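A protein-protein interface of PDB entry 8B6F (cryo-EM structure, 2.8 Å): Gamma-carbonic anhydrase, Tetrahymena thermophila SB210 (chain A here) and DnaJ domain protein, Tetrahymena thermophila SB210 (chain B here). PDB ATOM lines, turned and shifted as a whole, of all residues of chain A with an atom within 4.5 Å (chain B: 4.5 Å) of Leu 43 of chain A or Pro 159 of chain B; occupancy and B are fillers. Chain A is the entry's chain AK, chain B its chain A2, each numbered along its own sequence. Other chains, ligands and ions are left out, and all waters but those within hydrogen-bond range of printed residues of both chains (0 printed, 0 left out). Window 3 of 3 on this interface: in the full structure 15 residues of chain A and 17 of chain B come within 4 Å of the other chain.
OG of Ser 42 of chain A sits at hydrogen-bond distance from O of Leu 46 of chain A, at 2.7 Å.
Among the printed residues, merely in contact across the chains: Asp 83 of chain A with Pro 159 of chain B, Asp 83 of chain A with Gly 157 of chain B, Leu 46 of chain A with Pro 159 of chain B, Tyr 44 of chain A with Lys 161 of chain B and Leu 43 of chain A with Pro 159 of chain B.
Leu 43 of chain A touches just one residue of chain B: Pro 159. Of the printed residues of chain B, Asp 83 of chain A touches Gly 157 (3.7 Å) and Pro 159 (3.3 Å). Pro 159 of chain B touches just these residues of chain A: Leu 43 (3.97 Å), Leu 46 (3.7 Å) and Asp 83 (3.3 Å). Printed residues of chain A within 4 Å of Val 160 of chain B: Asp 45 (3.2 Å). Printed residues of chain A within 4 Å of Lys 161 of chain B: Tyr 44 (3.9 Å). The nearest printed residue of chain B that does not touch Leu 43 of chain A is Val 160 of chain B (5.2 Å). The nearest printed residue of chain B that does not touch Leu 46 of chain A is Val 160 of chain B (6.6 Å).
The side-chain carboxylate of Asp 45 of chain A sits close to the backbone carbonyl oxygen of Val 160 of chain B (3.2 Å).
Printed residues of chain B that touch a printed residue of chain A: Gly 157, Pro 159, Val 160 and Lys 161. Among the printed residues, 6 pairs touch across the chains. Among the printed residues, no Asp or Glu carboxylate lies within 4 Å of a Lys or Arg side-chain nitrogen of the other chain.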
ATOM      1  N   SER A  42      20.972   1.666  14.003  1.00  0.00           N
ATOM      2  CA  SER A  42      21.598   0.355  14.075  1.00  0.00           C
ATOM      3  C   SER A  42      22.081   0.117  15.498  1.00  0.00           C
ATOM      4  O   SER A  42      22.308   1.061  16.256  1.00  0.00           O
ATOM      5  CB  SER A  42      22.768   0.250  13.089  1.00  0.00           C
ATOM      6  OG  SER A  42      23.580  -0.873  13.378  1.00  0.00           O
ATOM      7  N   LEU A  43      22.241  -1.156  15.862  1.00  0.00           N
ATOM      8  CA  LEU A  43      22.790  -1.518  17.169  1.00  0.00           C
ATOM      9  C   LEU A  43      24.062  -2.334  16.954  1.00  0.00           C
ATOM     10  O   LEU A  43      24.071  -3.563  17.045  1.00  0.00           O
ATOM     11  CB  LEU A  43      21.752  -2.287  17.980  1.00  0.00           C
ATOM     12  CG  LEU A  43      20.383  -1.614  18.107  1.00  0.00           C
ATOM     13  CD1 LEU A  43      19.400  -2.520  18.826  1.00  0.00           C
ATOM     14  CD2 LEU A  43      20.507  -0.286  18.832  1.00  0.00           C
ATOM     15  N   TYR A  44      25.145  -1.618  16.667  1.00  0.00           N
ATOM     16  CA  TYR A  44      26.535  -2.062  16.716  1.00  0.00           C
ATOM     17  C   TYR A  44      26.894  -3.092  15.652  1.00  0.00           C
ATOM     18  O   TYR A  44      28.077  -3.274  15.347  1.00  0.00           O
ATOM     19  CB  TYR A  44      26.857  -2.682  18.083  1.00  0.00           C
ATOM     20  CG  TYR A  44      26.279  -1.966  19.282  1.00  0.00           C
ATOM     21  CD1 TYR A  44      26.128  -0.584  19.293  1.00  0.00           C
ATOM     22  CD2 TYR A  44      25.894  -2.678  20.411  1.00  0.00           C
ATOM     23  CE1 TYR A  44      25.601   0.066  20.391  1.00  0.00           C
ATOM     24  CE2 TYR A  44      25.367  -2.040  21.512  1.00  0.00           C
ATOM     25  CZ  TYR A  44      25.222  -0.666  21.497  1.00  0.00           C
ATOM     26  OH  TYR A  44      24.699  -0.020  22.593  1.00  0.00           O
ATOM     27  N   ASP A  45      25.904  -3.758  15.068  1.00  0.00           N
ATOM     28  CA  ASP A  45      26.150  -4.585  13.894  1.00  0.00           C
ATOM     29  C   ASP A  45      24.960  -4.670  12.955  1.00  0.00           C
ATOM     30  O   ASP A  45      25.058  -5.367  11.942  1.00  0.00           O
ATOM     31  CB  ASP A  45      26.563  -5.997  14.332  1.00  0.00           C
ATOM     32  CG  ASP A  45      27.960  -6.040  14.910  1.00  0.00           C
ATOM     33  OD1 ASP A  45      28.877  -5.458  14.294  1.00  0.00           O
ATOM     34  OD2 ASP A  45      28.138  -6.646  15.987  1.00  0.00           O
ATOM     35  N   LEU A  46      23.850  -4.000  13.242  1.00  0.00           N
ATOM     36  CA  LEU A  46      22.562  -4.303  12.628  1.00  0.00           C
ATOM     37  C   LEU A  46      22.131  -3.088  11.820  1.00  0.00           C
ATOM     38  O   LEU A  46      21.460  -2.190  12.332  1.00  0.00           O
ATOM     39  CB  LEU A  46      21.532  -4.671  13.692  1.00  0.00           C
ATOM     40  CG  LEU A  46      21.985  -5.701  14.732  1.00  0.00           C
ATOM     41  CD1 LEU A  46      20.879  -5.956  15.735  1.00  0.00           C
ATOM     42  CD2 LEU A  46      22.415  -7.002  14.077  1.00  0.00           C
ATOM     43  N   ILE A  63      14.793   0.457  13.159  1.00  0.00           N
ATOM     44  CA  ILE A  63      16.036   0.259  13.891  1.00  0.00           C
ATOM     45  C   ILE A  63      16.342  -1.229  13.956  1.00  0.00           C
ATOM     46  O   ILE A  63      15.444  -2.048  14.179  1.00  0.00           O
ATOM     47  CB  ILE A  63      15.959   0.865  15.307  1.00  0.00           C
ATOM     48  CG1 ILE A  63      17.291   0.678  16.033  1.00  0.00           C
ATOM     49  CG2 ILE A  63      14.817   0.241  16.096  1.00  0.00           C
ATOM     50  CD1 ILE A  63      17.398   1.455  17.321  1.00  0.00           C
ATOM     51  N   ASP A  83      15.896  -5.629  16.361  1.00  0.00           N
ATOM     52  CA  ASP A  83      17.001  -5.714  17.310  1.00  0.00           C
ATOM     53  C   ASP A  83      17.127  -7.114  17.902  1.00  0.00           C
ATOM     54  O   ASP A  83      18.237  -7.647  18.009  1.00  0.00           O
ATOM     55  CB  ASP A  83      16.815  -4.663  18.402  1.00  0.00           C
ATOM     56  CG  ASP A  83      15.428  -4.690  19.008  1.00  0.00           C
ATOM     57  OD1 ASP A  83      14.650  -5.605  18.669  1.00  0.00           O
ATOM     58  OD2 ASP A  83      15.100  -3.775  19.790  1.00  0.00           O
ATOM     59  N   GLY B 157      18.418 -12.612  20.660  1.00  0.00           N
ATOM     60  CA  GLY B 157      18.519 -11.948  21.951  1.00  0.00           C
ATOM     61  C   GLY B 157      19.135 -10.574  21.822  1.00  0.00           C
ATOM     62  O   GLY B 157      19.032  -9.924  20.776  1.00  0.00           O
ATOM     63  N   LEU B 158      19.774 -10.143  22.897  1.00  0.00           N
ATOM     64  CA  LEU B 158      20.382  -8.821  22.919  1.00  0.00           C
ATOM     65  C   LEU B 158      21.520  -8.752  21.907  1.00  0.00           C
ATOM     66  O   LEU B 158      22.382  -9.637  21.895  1.00  0.00           O
ATOM     67  CB  LEU B 158      20.910  -8.510  24.316  1.00  0.00           C
ATOM     68  CG  LEU B 158      19.900  -8.645  25.455  1.00  0.00           C
ATOM     69  CD1 LEU B 158      20.593  -8.476  26.790  1.00  0.00           C
ATOM     70  CD2 LEU B 158      18.777  -7.635  25.300  1.00  0.00           C
ATOM     71  N   PRO B 159      21.562  -7.735  21.046  1.00  0.00           N
ATOM     72  CA  PRO B 159      22.720  -7.588  20.157  1.00  0.00           C
ATOM     73  C   PRO B 159      24.003  -7.421  20.956  1.00  0.00           C
ATOM     74  O   PRO B 159      24.017  -6.801  22.020  1.00  0.00           O
ATOM     75  CB  PRO B 159      22.391  -6.330  19.346  1.00  0.00           C
ATOM     76  CG  PRO B 159      20.914  -6.211  19.410  1.00  0.00           C
ATOM     77  CD  PRO B 159      20.516  -6.741  20.752  1.00  0.00           C
ATOM     78  N   VAL B 160      25.085  -7.985  20.431  1.00  0.00           N
ATOM     79  CA  VAL B 160      26.392  -7.947  21.075  1.00  0.00           C
ATOM     80  C   VAL B 160      27.310  -7.056  20.252  1.00  0.00           C
ATOM     81  O   VAL B 160      27.332  -7.139  19.019  1.00  0.00           O
ATOM     82  CB  VAL B 160      26.990  -9.357  21.238  1.00  0.00           C
ATOM     83  CG1 VAL B 160      28.356  -9.278  21.893  1.00  0.00           C
ATOM     84  CG2 VAL B 160      26.059 -10.241  22.048  1.00  0.00           C
ATOM     85  N   LYS B 161      28.067  -6.205  20.935  1.00  0.00           N
ATOM     86  CA  LYS B 161      28.928  -5.244  20.260  1.00  0.00           C
ATOM     87  C   LYS B 161      30.126  -5.957  19.645  1.00  0.00           C
ATOM     88  O   LYS B 161      30.889  -6.626  20.349  1.00  0.00           O
ATOM     89  CB  LYS B 161      29.388  -4.175  21.246  1.00  0.00           C
ATOM     90  CG  LYS B 161      30.246  -3.084  20.630  1.00  0.00           C
ATOM     91  CD  LYS B 161      30.647  -2.055  21.675  1.00  0.00           C
ATOM     92  CE  LYS B 161      31.500  -0.953  21.068  1.00  0.00           C
ATOM     93  NZ  LYS B 161      31.914   0.054  22.084  1.00  0.00           N
